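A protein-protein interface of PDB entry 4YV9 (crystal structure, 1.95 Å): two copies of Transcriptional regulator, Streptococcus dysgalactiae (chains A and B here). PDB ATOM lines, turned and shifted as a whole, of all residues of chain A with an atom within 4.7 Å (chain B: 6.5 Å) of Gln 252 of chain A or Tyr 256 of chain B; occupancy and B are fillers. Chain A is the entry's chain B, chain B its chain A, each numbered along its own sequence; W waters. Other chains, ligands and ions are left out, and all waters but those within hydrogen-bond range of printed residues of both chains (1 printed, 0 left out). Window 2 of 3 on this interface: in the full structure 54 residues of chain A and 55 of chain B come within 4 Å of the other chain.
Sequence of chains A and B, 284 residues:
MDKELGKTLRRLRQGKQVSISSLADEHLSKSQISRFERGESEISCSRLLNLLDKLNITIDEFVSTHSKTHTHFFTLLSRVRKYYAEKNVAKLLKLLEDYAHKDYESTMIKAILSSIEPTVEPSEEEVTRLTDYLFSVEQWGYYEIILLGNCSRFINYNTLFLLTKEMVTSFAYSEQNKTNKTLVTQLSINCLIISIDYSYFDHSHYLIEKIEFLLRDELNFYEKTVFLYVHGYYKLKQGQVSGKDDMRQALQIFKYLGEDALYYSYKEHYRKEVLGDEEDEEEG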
ATOM      1  N   LEU A 228       7.924 -21.731  22.134  1.00  0.00           N
ATOM      2  CA  LEU A 228       8.308 -20.642  21.226  1.00  0.00           C
ATOM      3  C   LEU A 228       9.280 -21.178  20.175  1.00  0.00           C
ATOM      4  O   LEU A 228       9.174 -20.868  18.995  1.00  0.00           O
ATOM      5  CB  LEU A 228       8.953 -19.486  21.997  1.00  0.00           C
ATOM      6  CG  LEU A 228       9.467 -18.302  21.183  1.00  0.00           C
ATOM      7  CD1 LEU A 228       8.341 -17.676  20.385  1.00  0.00           C
ATOM      8  CD2 LEU A 228      10.073 -17.290  22.138  1.00  0.00           C
ATOM      9  N   ARG A 248      15.255 -17.733  17.517  1.00  0.00           N
ATOM     10  CA  ARG A 248      16.330 -16.901  18.062  1.00  0.00           C
ATOM     11  C   ARG A 248      15.906 -16.222  19.377  1.00  0.00           C
ATOM     12  O   ARG A 248      16.721 -16.055  20.277  1.00  0.00           O
ATOM     13  CB  ARG A 248      16.782 -15.861  17.040  1.00  0.00           C
ATOM     14  CG  ARG A 248      17.857 -16.396  16.102  1.00  0.00           C
ATOM     15  CD  ARG A 248      18.224 -15.386  15.021  1.00  0.00           C
ATOM     16  NE  ARG A 248      17.029 -14.897  14.339  1.00  0.00           N
ATOM     17  CZ  ARG A 248      17.008 -14.460  13.085  1.00  0.00           C
ATOM     18  NH1 ARG A 248      18.124 -14.443  12.363  1.00  0.00           N
ATOM     19  NH2 ARG A 248      15.869 -14.040  12.554  1.00  0.00           N
ATOM     20  N   GLN A 249      14.633 -15.836  19.483  1.00  0.00           N
ATOM     21  CA  GLN A 249      14.110 -15.271  20.732  1.00  0.00           C
ATOM     22  C   GLN A 249      14.159 -16.286  21.876  1.00  0.00           C
ATOM     23  O   GLN A 249      14.553 -15.958  23.002  1.00  0.00           O
ATOM     24  CB  GLN A 249      12.673 -14.769  20.531  1.00  0.00           C
ATOM     25  CG  GLN A 249      12.589 -13.526  19.636  1.00  0.00           C
ATOM     26  CD  GLN A 249      11.162 -13.169  19.289  1.00  0.00           C
ATOM     27  OE1 GLN A 249      10.234 -13.813  19.756  1.00  0.00           O
ATOM     28  NE2 GLN A 249      10.980 -12.141  18.474  1.00  0.00           N
ATOM     29  N   ALA A 250      13.774 -17.524  21.585  1.00  0.00           N
ATOM     30  CA  ALA A 250      13.832 -18.578  22.596  1.00  0.00           C
ATOM     31  C   ALA A 250      15.261 -18.783  23.068  1.00  0.00           C
ATOM     32  O   ALA A 250      15.494 -18.951  24.260  1.00  0.00           O
ATOM     33  CB  ALA A 250      13.257 -19.882  22.060  1.00  0.00           C
ATOM     34  N   LEU A 251      16.220 -18.750  22.138  1.00  0.00           N
ATOM     35  CA  LEU A 251      17.626 -18.916  22.501  1.00  0.00           C
ATOM     36  C   LEU A 251      18.048 -17.819  23.470  1.00  0.00           C
ATOM     37  O   LEU A 251      18.717 -18.088  24.471  1.00  0.00           O
ATOM     38  CB  LEU A 251      18.538 -18.891  21.258  1.00  0.00           C
ATOM     39  CG  LEU A 251      18.466 -20.074  20.289  1.00  0.00           C
ATOM     40  CD1 LEU A 251      19.413 -19.901  19.082  1.00  0.00           C
ATOM     41  CD2 LEU A 251      18.746 -21.376  21.016  1.00  0.00           C
ATOM     42  N   GLN A 252      17.671 -16.583  23.146  1.00  0.00           N
ATOM     43  CA  GLN A 252      17.969 -15.426  23.991  1.00  0.00           C
ATOM     44  C   GLN A 252      17.421 -15.608  25.409  1.00  0.00           C
ATOM     45  O   GLN A 252      18.081 -15.248  26.391  1.00  0.00           O
ATOM     46  CB  GLN A 252      17.381 -14.143  23.391  1.00  0.00           C
ATOM     47  CG  GLN A 252      18.033 -13.659  22.102  1.00  0.00           C
ATOM     48  CD  GLN A 252      17.383 -12.383  21.570  1.00  0.00           C
ATOM     49  OE1 GLN A 252      17.354 -11.354  22.250  1.00  0.00           O
ATOM     50  NE2 GLN A 252      16.853 -12.450  20.351  1.00  0.00           N
ATOM     51  N   ILE A 253      16.216 -16.162  25.515  1.00  0.00           N
ATOM     52  CA  ILE A 253      15.608 -16.405  26.830  1.00  0.00           C
ATOM     53  C   ILE A 253      16.495 -17.351  27.666  1.00  0.00           C
ATOM     54  O   ILE A 253      16.874 -17.020  28.788  1.00  0.00           O
ATOM     55  CB  ILE A 253      14.175 -16.982  26.687  1.00  0.00           C
ATOM     56  CG1 ILE A 253      13.263 -15.926  26.062  1.00  0.00           C
ATOM     57  CG2 ILE A 253      13.620 -17.404  28.042  1.00  0.00           C
ATOM     58  CD1 ILE A 253      11.858 -16.391  25.778  1.00  0.00           C
ATOM     59  N   PHE A 254      16.835 -18.517  27.118  1.00  0.00           N
ATOM     60  CA  PHE A 254      17.757 -19.444  27.789  1.00  0.00           C
ATOM     61  C   PHE A 254      19.040 -18.720  28.212  1.00  0.00           C
ATOM     62  O   PHE A 254      19.521 -18.880  29.336  1.00  0.00           O
ATOM     63  CB  PHE A 254      18.130 -20.620  26.877  1.00  0.00           C
ATOM     64  CG  PHE A 254      17.002 -21.565  26.577  1.00  0.00           C
ATOM     65  CD1 PHE A 254      16.115 -21.966  27.571  1.00  0.00           C
ATOM     66  CD2 PHE A 254      16.836 -22.069  25.296  1.00  0.00           C
ATOM     67  CE1 PHE A 254      15.082 -22.854  27.284  1.00  0.00           C
ATOM     68  CE2 PHE A 254      15.803 -22.944  25.003  1.00  0.00           C
ATOM     69  CZ  PHE A 254      14.925 -23.341  25.997  1.00  0.00           C
ATOM     70  N   LYS A 255      19.589 -17.937  27.285  1.00  0.00           N
ATOM     71  CA  LYS A 255      20.811 -17.177  27.509  1.00  0.00           C
ATOM     72  C   LYS A 255      20.674 -16.205  28.672  1.00  0.00           C
ATOM     73  O   LYS A 255      21.467 -16.230  29.616  1.00  0.00           O
ATOM     74  CB  LYS A 255      21.185 -16.409  26.245  1.00  0.00           C
ATOM     75  CG  LYS A 255      22.522 -15.697  26.303  1.00  0.00           C
ATOM     76  CD  LYS A 255      22.681 -14.856  25.044  1.00  0.00           C
ATOM     77  CE  LYS A 255      23.959 -14.050  25.033  1.00  0.00           C
ATOM     78  NZ  LYS A 255      24.005 -13.193  23.811  1.00  0.00           N
ATOM     79  N   TYR A 256      19.647 -15.362  28.591  1.00  0.00           N
ATOM     80  CA  TYR A 256      19.393 -14.339  29.590  1.00  0.00           C
ATOM     81  C   TYR A 256      19.199 -14.954  30.978  1.00  0.00           C
ATOM     82  O   TYR A 256      19.599 -14.355  31.965  1.00  0.00           O
ATOM     83  CB  TYR A 256      18.157 -13.495  29.202  1.00  0.00           C
ATOM     84  CG  TYR A 256      18.359 -12.582  28.004  1.00  0.00           C
ATOM     85  CD1 TYR A 256      19.624 -12.381  27.458  1.00  0.00           C
ATOM     86  CD2 TYR A 256      17.284 -11.911  27.420  1.00  0.00           C
ATOM     87  CE1 TYR A 256      19.815 -11.547  26.367  1.00  0.00           C
ATOM     88  CE2 TYR A 256      17.467 -11.067  26.329  1.00  0.00           C
ATOM     89  CZ  TYR A 256      18.735 -10.893  25.803  1.00  0.00           C
ATOM     90  OH  TYR A 256      18.934 -10.060  24.718  1.00  0.00           O
ATOM     91  N   LEU B 251      12.536  -7.894  30.669  1.00  0.00           N
ATOM     92  CA  LEU B 251      11.451  -7.297  29.885  1.00  0.00           C
ATOM     93  C   LEU B 251      11.364  -7.942  28.510  1.00  0.00           C
ATOM     94  O   LEU B 251      10.273  -8.171  27.990  1.00  0.00           O
ATOM     95  CB  LEU B 251      11.655  -5.789  29.729  1.00  0.00           C
ATOM     96  CG  LEU B 251      11.511  -4.979  31.011  1.00  0.00           C
ATOM     97  CD1 LEU B 251      11.882  -3.528  30.753  1.00  0.00           C
ATOM     98  CD2 LEU B 251      10.075  -5.104  31.565  1.00  0.00           C
ATOM     99  N   GLN B 252      12.522  -8.220  27.917  1.00  0.00           N
ATOM    100  CA  GLN B 252      12.553  -8.840  26.597  1.00  0.00           C
ATOM    101  C   GLN B 252      11.920 -10.215  26.669  1.00  0.00           C
ATOM    102  O   GLN B 252      11.156 -10.595  25.787  1.00  0.00           O
ATOM    103  CB  GLN B 252      13.985  -8.942  26.037  1.00  0.00           C
ATOM    104  CG  GLN B 252      14.563  -7.654  25.476  1.00  0.00           C
ATOM    105  CD  GLN B 252      13.727  -7.060  24.354  1.00  0.00           C
ATOM    106  OE1 GLN B 252      12.695  -6.432  24.597  1.00  0.00           O
ATOM    107  NE2 GLN B 252      14.177  -7.242  23.119  1.00  0.00           N
ATOM    108  N   ILE B 253      12.239 -10.955  27.725  1.00  0.00           N
ATOM    109  CA  ILE B 253      11.651 -12.275  27.944  1.00  0.00           C
ATOM    110  C   ILE B 253      10.110 -12.220  28.031  1.00  0.00           C
ATOM    111  O   ILE B 253       9.417 -13.004  27.375  1.00  0.00           O
ATOM    112  CB  ILE B 253      12.207 -12.916  29.226  1.00  0.00           C
ATOM    113  CG1 ILE B 253      13.700 -13.242  29.044  1.00  0.00           C
ATOM    114  CG2 ILE B 253      11.449 -14.186  29.568  1.00  0.00           C
ATOM    115  CD1 ILE B 253      14.375 -13.701  30.331  1.00  0.00           C
ATOM    116  N   PHE B 254       9.582 -11.301  28.834  1.00  0.00           N
ATOM    117  CA  PHE B 254       8.129 -11.101  28.878  1.00  0.00           C
ATOM    118  C   PHE B 254       7.610 -10.808  27.473  1.00  0.00           C
ATOM    119  O   PHE B 254       6.580 -11.339  27.054  1.00  0.00           O
ATOM    120  CB  PHE B 254       7.745  -9.951  29.817  1.00  0.00           C
ATOM    121  CG  PHE B 254       8.074 -10.193  31.255  1.00  0.00           C
ATOM    122  CD1 PHE B 254       7.911 -11.442  31.826  1.00  0.00           C
ATOM    123  CD2 PHE B 254       8.556  -9.164  32.040  1.00  0.00           C
ATOM    124  CE1 PHE B 254       8.199 -11.657  33.165  1.00  0.00           C
ATOM    125  CE2 PHE B 254       8.854  -9.375  33.375  1.00  0.00           C
ATOM    126  CZ  PHE B 254       8.667 -10.626  33.939  1.00  0.00           C
ATOM    127  N   LYS B 255       8.333  -9.967  26.735  1.00  0.00           N
ATOM    128  CA  LYS B 255       7.844  -9.558  25.428  1.00  0.00           C
ATOM    129  C   LYS B 255       7.815 -10.744  24.467  1.00  0.00           C
ATOM    130  O   LYS B 255       6.814 -10.968  23.783  1.00  0.00           O
ATOM    131  CB  LYS B 255       8.701  -8.427  24.838  1.00  0.00           C
ATOM    132  CG  LYS B 255       8.192  -7.979  23.486  1.00  0.00           C
ATOM    133  CD  LYS B 255       9.077  -6.940  22.816  1.00  0.00           C
ATOM    134  CE  LYS B 255       8.481  -6.552  21.471  1.00  0.00           C
ATOM    135  NZ  LYS B 255       9.056  -5.303  20.901  1.00  0.00           N
ATOM    136  N   TYR B 256       8.917 -11.497  24.417  1.00  0.00           N
ATOM    137  CA  TYR B 256       9.051 -12.637  23.506  1.00  0.00           C
ATOM    138  C   TYR B 256       7.974 -13.700  23.754  1.00  0.00           C
ATOM    139  O   TYR B 256       7.476 -14.331  22.818  1.00  0.00           O
ATOM    140  CB  TYR B 256      10.444 -13.274  23.638  1.00  0.00           C
ATOM    141  CG  TYR B 256      11.573 -12.385  23.159  1.00  0.00           C
ATOM    142  CD1 TYR B 256      11.312 -11.209  22.463  1.00  0.00           C
ATOM    143  CD2 TYR B 256      12.894 -12.727  23.389  1.00  0.00           C
ATOM    144  CE1 TYR B 256      12.347 -10.390  22.018  1.00  0.00           C
ATOM    145  CE2 TYR B 256      13.931 -11.923  22.945  1.00  0.00           C
ATOM    146  CZ  TYR B 256      13.656 -10.757  22.270  1.00  0.00           C
ATOM    147  OH  TYR B 256      14.690  -9.953  21.824  1.00  0.00           O
ATOM    148  N   LEU B 257       7.619 -13.896  25.012  1.00  0.00           N
ATOM    149  CA  LEU B 257       6.640 -14.924  25.361  1.00  0.00           C
ATOM    150  C   LEU B 257       5.208 -14.407  25.252  1.00  0.00           C
ATOM    151  O   LEU B 257       4.263 -15.130  25.569  1.00  0.00           O
ATOM    152  CB  LEU B 257       6.905 -15.453  26.769  1.00  0.00           C
ATOM    153  CG  LEU B 257       8.285 -16.118  26.970  1.00  0.00           C
ATOM    154  CD1 LEU B 257       8.435 -16.565  28.438  1.00  0.00           C
ATOM    155  CD2 LEU B 257       8.444 -17.289  26.040  1.00  0.00           C
ATOM    156  N   GLY B 258       5.050 -13.165  24.804  1.00  0.00           N
ATOM    157  CA  GLY B 258       3.719 -12.568  24.692  1.00  0.00           C
ATOM    158  C   GLY B 258       3.035 -12.384  26.034  1.00  0.00           C
ATOM    159  O   GLY B 258       1.800 -12.456  26.133  1.00  0.00           O
ATOM    160  N   GLU B 259       3.815 -12.158  27.088  1.00  0.00           N
ATOM    161  CA  GLU B 259       3.234 -11.972  28.426  1.00  0.00           C
ATOM    162  C   GLU B 259       2.932 -10.497  28.689  1.00  0.00           C
ATOM    163  O   GLU B 259       3.661  -9.817  29.425  1.00  0.00           O
ATOM    164  CB  GLU B 259       4.175 -12.518  29.503  1.00  0.00           C
ATOM    165  CG  GLU B 259       4.412 -14.024  29.404  1.00  0.00           C
ATOM    166  CD  GLU B 259       3.219 -14.825  29.925  1.00  0.00           C
ATOM    167  OE1 GLU B 259       2.548 -14.347  30.869  1.00  0.00           O
ATOM    168  OE2 GLU B 259       2.955 -15.928  29.394  1.00  0.00           O
ATOM    169  N   TYR B 263       4.979  -7.792  31.065  1.00  0.00           N
ATOM    170  CA  TYR B 263       5.775  -6.841  30.298  1.00  0.00           C
ATOM    171  C   TYR B 263       5.386  -5.379  30.616  1.00  0.00           C
ATOM    172  O   TYR B 263       6.244  -4.565  30.953  1.00  0.00           O
ATOM    173  CB  TYR B 263       5.599  -7.126  28.804  1.00  0.00           C
ATOM    174  CG  TYR B 263       6.268  -6.131  27.891  1.00  0.00           C
ATOM    175  CD1 TYR B 263       7.642  -6.179  27.678  1.00  0.00           C
ATOM    176  CD2 TYR B 263       5.536  -5.162  27.227  1.00  0.00           C
ATOM    177  CE1 TYR B 263       8.265  -5.280  26.830  1.00  0.00           C
ATOM    178  CE2 TYR B 263       6.153  -4.249  26.378  1.00  0.00           C
ATOM    179  CZ  TYR B 263       7.519  -4.317  26.188  1.00  0.00           C
ATOM    180  OH  TYR B 263       8.139  -3.422  25.356  1.00  0.00           O
HETATM  181  O   HOH W   1       7.781 -13.835  20.103  1.00  0.00           O
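Of the 10 printed residues of chain B, 3 touch a printed residue of chain A.
Along chain B the printed residues that touch a printed residue of chain A span positions 253 to 257.
Gln 252 of chain A touches Tyr 256 of chain B, but with the chains exchanged Tyr 256 of chain A does not touch Gln 252 of chain B (4.1 Å).
Tyr 256 of chain A touches Ile 253 of chain B, but with the chains exchanged Ile 253 of chain A does not touch Tyr 256 of chain B (4.04 Å).
Of chain B, only Tyr 256 (3.0 Å) comes within 4 Å of Gln 252 of chain A.
Printed residues of chain A within 4 Å of Tyr 256 of chain B: Leu 228 (3.995 Å), Gln 249 (3.5 Å) and Gln 252 (3.0 Å).
Printed residues of chain B within 4 Å of Leu 228 of chain A: Tyr 256.
Of the printed residues of chain B, Ile 253 of chain A touches Leu 257.
Of the printed residues of chain A, Ile 253 of chain B touches Tyr 256.
Printed residues of chain B within 4 Å of Gln 249 of chain A: Tyr 256 (3.5 Å).
The nearest residue of chain B that does not touch Gln 252 of chain A is Gln 252 of chain B (5.3 Å).
The nearest printed residue of chain A that does not touch Leu 257 of chain B is Leu 228 of chain A (4.2 Å).
The side-chain amide nitrogen (NE2) of Gln 252 of chain B is in hydrogen-bond range of the side-chain hydroxyl (OH) of Tyr 256 of chain B (3.0 Å).
The side-chain hydroxyl (OH) of Tyr 256 of chain A is in hydrogen-bond range of the side-chain amide oxygen (OE1) of Gln 252 of chain A.
Water W1 bridges the side-chain amide oxygen (OE1) of Gln 249 of chain A and the backbone carbonyl oxygen (O) of Tyr 256 of chain B.
CD2 of Leu 228 of chain A touches O of Tyr 256 of chain B, 3.995 Å away.
Gln 249 of chain A touches Tyr 256 of chain B.
Ile 253 of chain A touches Leu 257 of chain B.
Tyr 256 of chain A touches Ile 253 of chain B.
OH of Tyr 256 of chain B is in hydrogen-bond range of OE1 of Gln 252 of chain A.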
